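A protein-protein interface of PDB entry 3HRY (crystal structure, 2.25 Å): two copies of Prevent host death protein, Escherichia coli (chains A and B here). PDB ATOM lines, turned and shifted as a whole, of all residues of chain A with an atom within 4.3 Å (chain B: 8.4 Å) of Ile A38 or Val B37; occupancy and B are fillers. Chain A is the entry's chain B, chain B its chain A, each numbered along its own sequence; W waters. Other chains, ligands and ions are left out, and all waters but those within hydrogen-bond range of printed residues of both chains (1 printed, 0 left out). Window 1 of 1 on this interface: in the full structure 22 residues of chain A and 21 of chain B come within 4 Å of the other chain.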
ATOM      1  N   LEU A  17      19.260 -31.570  21.821  1.00  0.00           N
ATOM      2  CA  LEU A  17      20.345 -32.514  21.509  1.00  0.00           C
ATOM      3  C   LEU A  17      20.023 -33.953  21.968  1.00  0.00           C
ATOM      4  O   LEU A  17      20.381 -34.916  21.294  1.00  0.00           O
ATOM      5  CB  LEU A  17      21.695 -32.058  22.116  1.00  0.00           C
ATOM      6  CG  LEU A  17      22.561 -30.856  21.690  1.00  0.00           C
ATOM      7  CD1 LEU A  17      22.352 -30.490  20.240  1.00  0.00           C
ATOM      8  CD2 LEU A  17      22.297 -29.665  22.574  1.00  0.00           C
ATOM      9  N   VAL A  20      18.164 -35.334  19.417  1.00  0.00           N
ATOM     10  CA  VAL A  20      19.056 -35.424  18.263  1.00  0.00           C
ATOM     11  C   VAL A  20      19.923 -36.685  18.359  1.00  0.00           C
ATOM     12  O   VAL A  20      20.063 -37.450  17.397  1.00  0.00           O
ATOM     13  CB  VAL A  20      19.939 -34.150  18.174  1.00  0.00           C
ATOM     14  CG1 VAL A  20      21.196 -34.373  17.329  1.00  0.00           C
ATOM     15  CG2 VAL A  20      19.110 -32.974  17.657  1.00  0.00           C
ATOM     16  N   GLU A  24      16.552 -37.814  16.100  1.00  0.00           N
ATOM     17  CA  GLU A  24      15.765 -36.926  15.279  1.00  0.00           C
ATOM     18  C   GLU A  24      16.624 -35.959  14.432  1.00  0.00           C
ATOM     19  O   GLU A  24      17.700 -35.579  14.799  1.00  0.00           O
ATOM     20  CB  GLU A  24      14.896 -36.119  16.251  1.00  0.00           C
ATOM     21  CG  GLU A  24      13.602 -35.510  15.753  1.00  0.00           C
ATOM     22  CD  GLU A  24      12.583 -36.516  15.294  1.00  0.00           C
ATOM     23  OE1 GLU A  24      11.777 -36.960  16.111  1.00  0.00           O
ATOM     24  OE2 GLU A  24      12.583 -36.848  14.098  1.00  0.00           O
ATOM     25  N   GLU A  25      16.115 -35.570  13.287  1.00  0.00           N
ATOM     26  CA  GLU A  25      16.601 -34.433  12.570  1.00  0.00           C
ATOM     27  C   GLU A  25      15.689 -33.310  12.974  1.00  0.00           C
ATOM     28  O   GLU A  25      14.551 -33.266  12.615  1.00  0.00           O
ATOM     29  CB  GLU A  25      16.526 -34.659  11.066  1.00  0.00           C
ATOM     30  CG  GLU A  25      16.289 -36.090  10.636  1.00  0.00           C
ATOM     31  CD  GLU A  25      16.693 -36.391   9.199  1.00  0.00           C
ATOM     32  OE1 GLU A  25      17.577 -37.237   8.992  1.00  0.00           O
ATOM     33  OE2 GLU A  25      16.119 -35.798   8.278  1.00  0.00           O
ATOM     34  N   VAL A  26      16.199 -32.407  13.764  1.00  0.00           N
ATOM     35  CA  VAL A  26      15.477 -31.233  14.236  1.00  0.00           C
ATOM     36  C   VAL A  26      15.759 -30.022  13.352  1.00  0.00           C
ATOM     37  O   VAL A  26      16.910 -29.742  13.016  1.00  0.00           O
ATOM     38  CB  VAL A  26      15.843 -30.891  15.691  1.00  0.00           C
ATOM     39  CG1 VAL A  26      15.355 -29.495  16.048  1.00  0.00           C
ATOM     40  CG2 VAL A  26      15.260 -31.926  16.642  1.00  0.00           C
ATOM     41  N   ILE A  28      15.603 -25.957  12.957  1.00  0.00           N
ATOM     42  CA  ILE A  28      15.507 -24.695  13.679  1.00  0.00           C
ATOM     43  C   ILE A  28      15.188 -23.535  12.742  1.00  0.00           C
ATOM     44  O   ILE A  28      16.069 -23.007  12.072  1.00  0.00           O
ATOM     45  CB  ILE A  28      16.810 -24.408  14.449  1.00  0.00           C
ATOM     46  CG1 ILE A  28      16.962 -25.406  15.598  1.00  0.00           C
ATOM     47  CG2 ILE A  28      16.853 -22.961  14.957  1.00  0.00           C
ATOM     48  CD1 ILE A  28      18.272 -25.295  16.326  1.00  0.00           C
ATOM     49  N   VAL A  37      18.882 -27.395  10.151  1.00  0.00           N
ATOM     50  CA  VAL A  37      18.602 -28.749  10.572  1.00  0.00           C
ATOM     51  C   VAL A  37      19.684 -29.193  11.508  1.00  0.00           C
ATOM     52  O   VAL A  37      20.841 -29.248  11.118  1.00  0.00           O
ATOM     53  CB  VAL A  37      18.630 -29.708   9.404  1.00  0.00           C
ATOM     54  CG1 VAL A  37      17.954 -30.990   9.808  1.00  0.00           C
ATOM     55  CG2 VAL A  37      17.914 -29.112   8.238  1.00  0.00           C
ATOM     56  N   ILE A  38      19.320 -29.514  12.742  1.00  0.00           N
ATOM     57  CA  ILE A  38      20.296 -30.063  13.669  1.00  0.00           C
ATOM     58  C   ILE A  38      20.167 -31.573  13.813  1.00  0.00           C
ATOM     59  O   ILE A  38      19.212 -32.072  14.389  1.00  0.00           O
ATOM     60  CB  ILE A  38      20.231 -29.383  15.036  1.00  0.00           C
ATOM     61  CG1 ILE A  38      21.155 -30.086  16.037  1.00  0.00           C
ATOM     62  CG2 ILE A  38      18.829 -29.346  15.535  1.00  0.00           C
ATOM     63  CD1 ILE A  38      21.588 -29.198  17.212  1.00  0.00           C
ATOM     64  N   VAL A  39      21.151 -32.288  13.277  1.00  0.00           N
ATOM     65  CA  VAL A  39      21.151 -33.742  13.249  1.00  0.00           C
ATOM     66  C   VAL A  39      22.456 -34.188  13.874  1.00  0.00           C
ATOM     67  O   VAL A  39      23.429 -33.444  13.860  1.00  0.00           O
ATOM     68  CB  VAL A  39      21.100 -34.255  11.808  1.00  0.00           C
ATOM     69  CG1 VAL A  39      22.259 -33.686  11.004  1.00  0.00           C
ATOM     70  CG2 VAL A  39      21.116 -35.772  11.782  1.00  0.00           C
ATOM     71  N   LYS A  41      26.052 -35.425  14.716  1.00  0.00           N
ATOM     72  CA  LYS A  41      27.241 -35.434  13.870  1.00  0.00           C
ATOM     73  C   LYS A  41      27.437 -36.805  13.245  1.00  0.00           C
ATOM     74  O   LYS A  41      27.577 -36.933  12.027  1.00  0.00           O
ATOM     75  CB  LYS A  41      28.523 -35.104  14.640  1.00  0.00           C
ATOM     76  CG  LYS A  41      29.792 -35.465  13.862  1.00  0.00           C
ATOM     77  CD  LYS A  41      31.051 -34.955  14.561  1.00  0.00           C
ATOM     78  CE  LYS A  41      32.291 -35.670  14.055  1.00  0.00           C
ATOM     79  NZ  LYS A  41      33.459 -35.378  14.937  1.00  0.00           N
ATOM     80  N   PHE A  44      25.249 -37.198  10.004  1.00  0.00           N
ATOM     81  CA  PHE A  44      25.556 -36.360   8.861  1.00  0.00           C
ATOM     82  C   PHE A  44      26.907 -36.750   8.261  1.00  0.00           C
ATOM     83  O   PHE A  44      27.061 -36.793   7.043  1.00  0.00           O
ATOM     84  CB  PHE A  44      25.546 -34.876   9.225  1.00  0.00           C
ATOM     85  CG  PHE A  44      26.040 -33.984   8.116  1.00  0.00           C
ATOM     86  CD1 PHE A  44      25.247 -33.729   7.007  1.00  0.00           C
ATOM     87  CD2 PHE A  44      27.299 -33.412   8.177  1.00  0.00           C
ATOM     88  CE1 PHE A  44      25.696 -32.923   5.987  1.00  0.00           C
ATOM     89  CE2 PHE A  44      27.753 -32.602   7.161  1.00  0.00           C
ATOM     90  CZ  PHE A  44      26.951 -32.352   6.064  1.00  0.00           C
ATOM     91  N   MET B   1      35.060 -27.024   9.169  1.00  0.00           N
ATOM     92  CA  MET B   1      33.892 -27.170  10.018  1.00  0.00           C
ATOM     93  C   MET B   1      34.151 -26.634  11.421  1.00  0.00           C
ATOM     94  O   MET B   1      34.968 -27.180  12.146  1.00  0.00           O
ATOM     95  CB  MET B   1      33.468 -28.637  10.045  1.00  0.00           C
ATOM     96  CG  MET B   1      32.768 -29.098  11.284  1.00  0.00           C
ATOM     97  SD  MET B   1      31.966 -30.660  10.969  1.00  0.00           S
ATOM     98  CE  MET B   1      31.905 -31.403  12.592  1.00  0.00           C
ATOM     99  N   GLN B   2      33.448 -25.564  11.779  1.00  0.00           N
ATOM    100  CA  GLN B   2      33.496 -24.899  13.074  1.00  0.00           C
ATOM    101  C   GLN B   2      33.018 -25.864  14.171  1.00  0.00           C
ATOM    102  O   GLN B   2      32.135 -26.686  13.931  1.00  0.00           O
ATOM    103  CB  GLN B   2      32.631 -23.638  13.034  1.00  0.00           C
ATOM    104  CG  GLN B   2      33.050 -22.557  14.015  1.00  0.00           C
ATOM    105  CD  GLN B   2      32.322 -21.258  13.773  1.00  0.00           C
ATOM    106  OE1 GLN B   2      31.578 -21.126  12.797  1.00  0.00           O
ATOM    107  NE2 GLN B   2      32.530 -20.283  14.660  1.00  0.00           N
ATOM    108  N   SER B   3      33.613 -25.790  15.358  1.00  0.00           N
ATOM    109  CA  SER B   3      33.216 -26.676  16.450  1.00  0.00           C
ATOM    110  C   SER B   3      33.087 -25.922  17.761  1.00  0.00           C
ATOM    111  O   SER B   3      34.071 -25.371  18.255  1.00  0.00           O
ATOM    112  CB  SER B   3      34.222 -27.810  16.626  1.00  0.00           C
ATOM    113  OG  SER B   3      33.869 -28.582  17.760  1.00  0.00           O
ATOM    114  N   ILE B   4      31.894 -25.898  18.348  1.00  0.00           N
ATOM    115  CA  ILE B   4      31.646 -25.195  19.605  1.00  0.00           C
ATOM    116  C   ILE B   4      30.996 -26.101  20.641  1.00  0.00           C
ATOM    117  O   ILE B   4      30.540 -27.145  20.320  1.00  0.00           O
ATOM    118  CB  ILE B   4      30.815 -23.923  19.379  1.00  0.00           C
ATOM    119  CG1 ILE B   4      29.410 -24.243  18.894  1.00  0.00           C
ATOM    120  CG2 ILE B   4      31.487 -23.043  18.368  1.00  0.00           C
ATOM    121  CD1 ILE B   4      28.770 -23.149  18.151  1.00  0.00           C
ATOM    122  N   ALA B   9      26.942 -22.523  22.183  1.00  0.00           N
ATOM    123  CA  ALA B   9      25.818 -22.701  21.267  1.00  0.00           C
ATOM    124  C   ALA B   9      24.507 -22.120  21.827  1.00  0.00           C
ATOM    125  O   ALA B   9      23.817 -21.360  21.141  1.00  0.00           O
ATOM    126  CB  ALA B   9      25.649 -24.175  20.938  1.00  0.00           C
ATOM    127  N   LEU B  13      23.766 -18.811  19.592  1.00  0.00           N
ATOM    128  CA  LEU B  13      23.044 -19.561  18.554  1.00  0.00           C
ATOM    129  C   LEU B  13      22.566 -18.721  17.372  1.00  0.00           C
ATOM    130  O   LEU B  13      22.631 -19.154  16.219  1.00  0.00           O
ATOM    131  CB  LEU B  13      21.812 -20.224  19.170  1.00  0.00           C
ATOM    132  CG  LEU B  13      21.079 -21.265  18.326  1.00  0.00           C
ATOM    133  CD1 LEU B  13      21.463 -22.648  18.825  1.00  0.00           C
ATOM    134  CD2 LEU B  13      19.563 -21.085  18.378  1.00  0.00           C
ATOM    135  N   LEU B  17      23.595 -19.389  13.516  1.00  0.00           N
ATOM    136  CA  LEU B  17      22.744 -19.759  12.410  1.00  0.00           C
ATOM    137  C   LEU B  17      23.043 -18.865  11.215  1.00  0.00           C
ATOM    138  O   LEU B  17      22.913 -19.280  10.064  1.00  0.00           O
ATOM    139  CB  LEU B  17      21.281 -19.662  12.841  1.00  0.00           C
ATOM    140  CG  LEU B  17      20.965 -20.510  14.078  1.00  0.00           C
ATOM    141  CD1 LEU B  17      19.477 -20.565  14.396  1.00  0.00           C
ATOM    142  CD2 LEU B  17      21.495 -21.904  13.865  1.00  0.00           C
ATOM    143  N   VAL B  20      25.823 -20.806   9.749  1.00  0.00           N
ATOM    144  CA  VAL B  20      25.517 -22.045   9.055  1.00  0.00           C
ATOM    145  C   VAL B  20      24.750 -21.711   7.787  1.00  0.00           C
ATOM    146  O   VAL B  20      24.744 -22.478   6.821  1.00  0.00           O
ATOM    147  CB  VAL B  20      24.733 -23.045   9.952  1.00  0.00           C
ATOM    148  CG1 VAL B  20      24.365 -24.305   9.167  1.00  0.00           C
ATOM    149  CG2 VAL B  20      25.553 -23.396  11.195  1.00  0.00           C
ATOM    150  N   GLU B  24      28.671 -22.816   6.794  1.00  0.00           N
ATOM    151  CA  GLU B  24      29.303 -23.481   7.922  1.00  0.00           C
ATOM    152  C   GLU B  24      28.481 -24.643   8.488  1.00  0.00           C
ATOM    153  O   GLU B  24      27.245 -24.684   8.418  1.00  0.00           O
ATOM    154  CB  GLU B  24      29.678 -22.472   9.027  1.00  0.00           C
ATOM    155  N   GLU B  25      29.213 -25.595   9.042  1.00  0.00           N
ATOM    156  CA  GLU B  25      28.648 -26.690   9.790  1.00  0.00           C
ATOM    157  C   GLU B  25      29.245 -26.602  11.183  1.00  0.00           C
ATOM    158  O   GLU B  25      30.447 -26.765  11.355  1.00  0.00           O
ATOM    159  CB  GLU B  25      29.018 -28.009   9.122  1.00  0.00           C
ATOM    160  CG  GLU B  25      28.686 -28.038   7.632  1.00  0.00           C
ATOM    161  CD  GLU B  25      29.390 -29.163   6.888  1.00  0.00           C
ATOM    162  OE1 GLU B  25      30.346 -29.742   7.453  1.00  0.00           O
ATOM    163  OE2 GLU B  25      28.987 -29.466   5.739  1.00  0.00           O
ATOM    164  N   VAL B  26      28.396 -26.342  12.174  1.00  0.00           N
ATOM    165  CA  VAL B  26      28.845 -26.076  13.536  1.00  0.00           C
ATOM    166  C   VAL B  26      28.528 -27.240  14.475  1.00  0.00           C
ATOM    167  O   VAL B  26      27.366 -27.552  14.714  1.00  0.00           O
ATOM    168  CB  VAL B  26      28.208 -24.770  14.076  1.00  0.00           C
ATOM    169  CG1 VAL B  26      28.573 -24.548  15.536  1.00  0.00           C
ATOM    170  CG2 VAL B  26      28.625 -23.583  13.224  1.00  0.00           C
ATOM    171  N   GLU B  27      29.577 -27.851  15.024  1.00  0.00           N
ATOM    172  CA  GLU B  27      29.479 -29.078  15.821  1.00  0.00           C
ATOM    173  C   GLU B  27      29.281 -28.850  17.325  1.00  0.00           C
ATOM    174  O   GLU B  27      30.252 -28.722  18.067  1.00  0.00           O
ATOM    175  CB  GLU B  27      30.743 -29.922  15.598  1.00  0.00           C
ATOM    176  CG  GLU B  27      30.936 -31.128  16.523  1.00  0.00           C
ATOM    177  CD  GLU B  27      32.315 -31.788  16.356  1.00  0.00           C
ATOM    178  OE1 GLU B  27      33.239 -31.131  15.818  1.00  0.00           O
ATOM    179  OE2 GLU B  27      32.472 -32.969  16.760  1.00  0.00           O
ATOM    180  N   ILE B  28      28.067 -28.807  17.804  1.00  0.00           N
ATOM    181  CA  ILE B  28      27.830 -28.597  19.209  1.00  0.00           C
ATOM    182  C   ILE B  28      28.216 -29.823  20.018  1.00  0.00           C
ATOM    183  O   ILE B  28      27.514 -30.800  20.002  1.00  0.00           O
ATOM    184  CB  ILE B  28      26.359 -28.316  19.434  1.00  0.00           C
ATOM    185  CG1 ILE B  28      25.817 -27.475  18.314  1.00  0.00           C
ATOM    186  CG2 ILE B  28      26.158 -27.549  20.643  1.00  0.00           C
ATOM    187  CD1 ILE B  28      24.879 -26.496  18.790  1.00  0.00           C
ATOM    188  N   THR B  29      29.338 -29.764  20.719  1.00  0.00           N
ATOM    189  CA  THR B  29      29.813 -30.850  21.560  1.00  0.00           C
ATOM    190  C   THR B  29      29.259 -30.712  22.973  1.00  0.00           C
ATOM    191  O   THR B  29      28.836 -29.631  23.368  1.00  0.00           O
ATOM    192  CB  THR B  29      31.324 -30.873  21.616  1.00  0.00           C
ATOM    193  OG1 THR B  29      31.800 -29.587  22.027  1.00  0.00           O
ATOM    194  CG2 THR B  29      31.896 -31.189  20.244  1.00  0.00           C
ATOM    195  N   GLU B  34      27.559 -37.352  23.064  1.00  0.00           N
ATOM    196  CA  GLU B  34      27.924 -37.435  21.658  1.00  0.00           C
ATOM    197  C   GLU B  34      27.477 -36.199  20.901  1.00  0.00           C
ATOM    198  O   GLU B  34      26.419 -35.637  21.188  1.00  0.00           O
ATOM    199  CB  GLU B  34      27.355 -38.702  21.024  1.00  0.00           C
ATOM    200  CG  GLU B  34      28.008 -39.984  21.541  1.00  0.00           C
ATOM    201  CD  GLU B  34      29.480 -40.069  21.180  1.00  0.00           C
ATOM    202  OE1 GLU B  34      29.828 -39.723  20.029  1.00  0.00           O
ATOM    203  OE2 GLU B  34      30.286 -40.482  22.044  1.00  0.00           O
ATOM    204  N   PRO B  35      28.283 -35.753  19.949  1.00  0.00           N
ATOM    205  CA  PRO B  35      28.171 -34.512  19.182  1.00  0.00           C
ATOM    206  C   PRO B  35      26.929 -34.322  18.270  1.00  0.00           C
ATOM    207  O   PRO B  35      26.576 -35.194  17.465  1.00  0.00           O
ATOM    208  CB  PRO B  35      29.465 -34.485  18.348  1.00  0.00           C
ATOM    209  CG  PRO B  35      29.999 -35.901  18.425  1.00  0.00           C
ATOM    210  CD  PRO B  35      29.638 -36.344  19.787  1.00  0.00           C
ATOM    211  N   ALA B  36      26.296 -33.156  18.417  1.00  0.00           N
ATOM    212  CA  ALA B  36      25.272 -32.673  17.495  1.00  0.00           C
ATOM    213  C   ALA B  36      25.870 -31.622  16.560  1.00  0.00           C
ATOM    214  O   ALA B  36      26.565 -30.708  16.993  1.00  0.00           O
ATOM    215  CB  ALA B  36      24.136 -32.079  18.257  1.00  0.00           C
ATOM    216  N   VAL B  37      25.587 -31.749  15.273  1.00  0.00           N
ATOM    217  CA  VAL B  37      26.102 -30.813  14.304  1.00  0.00           C
ATOM    218  C   VAL B  37      24.950 -30.100  13.650  1.00  0.00           C
ATOM    219  O   VAL B  37      23.834 -30.593  13.640  1.00  0.00           O
ATOM    220  CB  VAL B  37      26.898 -31.509  13.196  1.00  0.00           C
ATOM    221  CG1 VAL B  37      25.944 -32.131  12.188  1.00  0.00           C
ATOM    222  CG2 VAL B  37      27.809 -30.510  12.503  1.00  0.00           C
ATOM    223  N   ILE B  38      25.243 -28.938  13.078  1.00  0.00           N
ATOM    224  CA  ILE B  38      24.229 -28.095  12.464  1.00  0.00           C
ATOM    225  C   ILE B  38      24.639 -27.645  11.083  1.00  0.00           C
ATOM    226  O   ILE B  38      25.586 -26.887  10.918  1.00  0.00           O
ATOM    227  CB  ILE B  38      23.998 -26.833  13.267  1.00  0.00           C
ATOM    228  CG1 ILE B  38      23.749 -27.181  14.739  1.00  0.00           C
ATOM    229  CG2 ILE B  38      22.852 -26.043  12.645  1.00  0.00           C
ATOM    230  CD1 ILE B  38      24.190 -26.105  15.721  1.00  0.00           C
ATOM    231  N   VAL B  39      23.891 -28.109  10.098  1.00  0.00           N
ATOM    232  CA  VAL B  39      24.138 -27.789   8.713  1.00  0.00           C
ATOM    233  C   VAL B  39      22.842 -27.161   8.225  1.00  0.00           C
ATOM    234  O   VAL B  39      21.791 -27.464   8.762  1.00  0.00           O
ATOM    235  CB  VAL B  39      24.474 -29.075   7.932  1.00  0.00           C
ATOM    236  CG1 VAL B  39      23.311 -30.049   7.972  1.00  0.00           C
ATOM    237  CG2 VAL B  39      24.880 -28.753   6.511  1.00  0.00           C
ATOM    238  N   SER B  40      22.901 -26.268   7.244  1.00  0.00           N
ATOM    239  CA  SER B  40      21.679 -25.642   6.744  1.00  0.00           C
ATOM    240  C   SER B  40      20.744 -26.664   6.106  1.00  0.00           C
ATOM    241  O   SER B  40      21.153 -27.801   5.850  1.00  0.00           O
ATOM    242  CB  SER B  40      21.987 -24.674   5.596  1.00  0.00           C
ATOM    243  OG  SER B  40      22.475 -25.351   4.449  1.00  0.00           O
ATOM    244  N   LYS B  41      19.494 -26.268   5.854  1.00  0.00           N
ATOM    245  CA  LYS B  41      18.510 -27.222   5.322  1.00  0.00           C
ATOM    246  C   LYS B  41      18.818 -27.629   3.874  1.00  0.00           C
ATOM    247  O   LYS B  41      18.688 -28.801   3.527  1.00  0.00           O
ATOM    248  CB  LYS B  41      17.059 -26.723   5.469  1.00  0.00           C
ATOM    249  CG  LYS B  41      15.993 -27.849   5.482  1.00  0.00           C
ATOM    250  CD  LYS B  41      14.564 -27.305   5.320  1.00  0.00           C
ATOM    251  CE  LYS B  41      13.531 -28.422   5.144  1.00  0.00           C
ATOM    252  NZ  LYS B  41      12.400 -28.017   4.246  1.00  0.00           N
ATOM    253  N   PHE B  44      21.794 -29.857   3.819  1.00  0.00           N
ATOM    254  CA  PHE B  44      21.551 -31.068   4.605  1.00  0.00           C
ATOM    255  C   PHE B  44      20.715 -32.140   3.883  1.00  0.00           C
ATOM    256  O   PHE B  44      21.093 -33.320   3.872  1.00  0.00           O
ATOM    257  CB  PHE B  44      20.988 -30.757   5.997  1.00  0.00           C
ATOM    258  CG  PHE B  44      20.416 -31.958   6.685  1.00  0.00           C
ATOM    259  CD1 PHE B  44      21.235 -32.868   7.324  1.00  0.00           C
ATOM    260  CD2 PHE B  44      19.052 -32.195   6.669  1.00  0.00           C
ATOM    261  CE1 PHE B  44      20.701 -33.992   7.945  1.00  0.00           C
ATOM    262  CE2 PHE B  44      18.509 -33.318   7.288  1.00  0.00           C
ATOM    263  CZ  PHE B  44      19.334 -34.215   7.926  1.00  0.00           C
HETATM  264  O   HOH W   1      23.346 -35.397  19.935  1.00  0.00           O
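The backbone carbonyl oxygen (O) of Val B39 lies within hydrogen-bond range of the backbone NH (N) of Val A37 (3.2 Å).
The backbone carbonyl oxygen (O) of Pro B35 sits at hydrogen-bond distance from the backbone NH (N) of Lys A41 (2.8 Å).
N of Val B37 sits at hydrogen-bond distance from O of Val A39 (3.1 Å).
The side-chain amino group (NZ) of Lys A41 lies within salt-bridge range of the side-chain carboxylate (OE2) of Glu B27 (3.2 Å).
O of Glu B27 is in hydrogen-bond range of N of Ile B4 (3.3 Å).
The backbone NH of Ile B28 sits at hydrogen-bond distance from the backbone carbonyl oxygen of Ala B36 (2.6 Å).
The side-chain carboxylate of Glu B27 lies within hydrogen-bond range of the side-chain hydroxyl of Ser B3 (3.3 Å).
The backbone carbonyl oxygen (O) of Gln B2 lies within hydrogen-bond range of the backbone NH (N) of Glu B27 (3.0 Å).
The backbone NH (N) of Gln B2 lies within hydrogen-bond range of the backbone carbonyl oxygen (O) of Glu B25, 3.3 Å away.
O of Val B26 is in hydrogen-bond range of N of Ile B38 (3.0 Å).
Ala B36 touches Leu A17.
CG1 of Val A20 touches CB of Ala B36, at 3.8 Å.
OE2 of Glu A25 touches CE2 of Phe B44, at 3.6 Å.
Val A37 touches Ile B38.
Ala B36 touches Ile A38 (CB to CD1, 3.99 Å).
Ile A38 touches Val B37 (CA to O, 3.6 Å).
CG1 of Ile B38 touches CD1 of Ile A38, at 3.9 Å.
CE1 of Phe B44 touches CG1 of Val A39, at 3.4 Å.
Lys A41 touches Ala B36 (N to CA, 3.99 Å).
Lys A41 touches Val B37.
Of the printed residues of chain B, Ile A38 touches Ala B36, Val B37 and Ile B38.
Printed residues of chain B within 4 Å of Lys A41: Glu B27 (3.2 Å), Pro B35 (2.8 Å), Ala B36 (3.99 Å) and Val B37 (3.7 Å).
Ala B9 touches none of the printed residues of chain A.
Of the printed residues of chain A, Glu B25 touches Phe A44.
Val B37 touches just these residues of chain A: Ile A38, Val A39 and Lys A41.
The nearest printed residue of chain B that does not touch Ile A38 is Ile B28 (4.5 Å).
The nearest printed residue of chain A that does not touch Glu B27 is Leu A17 (7.7 Å).
Of the 11 printed residues of chain A, 9 touch a printed residue of chain B.
Printed residues of chain A that touch a printed residue of chain B: Leu A17, Val A20, Glu A25, Ile A28, Val A37, Ile A38, Val A39, Lys A41 and Phe A44.
Of the 23 printed residues of chain B, 10 touch a printed residue of chain A.
Hydrophobic or aromatic side chains of chain B within 4 Å of the printed part of chain A: Leu B17, Pro B35, Ala B36, Val B37, Ile B38 and Phe B44.
Along chain B the printed residues that touch a printed residue of chain A span positions 17 to 44.
Ile A28 touches Leu B17, but with the chains exchanged Leu A17 does not touch Ile B28 (4.6 Å).
Val A37 touches Lys B41, and with the chains exchanged Lys A41 touches Val B37.
Val A37 touches Phe B44, but with the chains exchanged Phe A44 does not touch Val B37 (4.1 Å).
Ile B38 touches its own counterpart, Ile A38.
11 positions are printed for both chains.
Of the 18 pairs that touch across the chains among the printed residues, 9 have their exchanged pair printed and touching as well.
Water W1 bridges O of Leu A17 (3.3 Å) and O of Glu B34 (3.3 Å).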
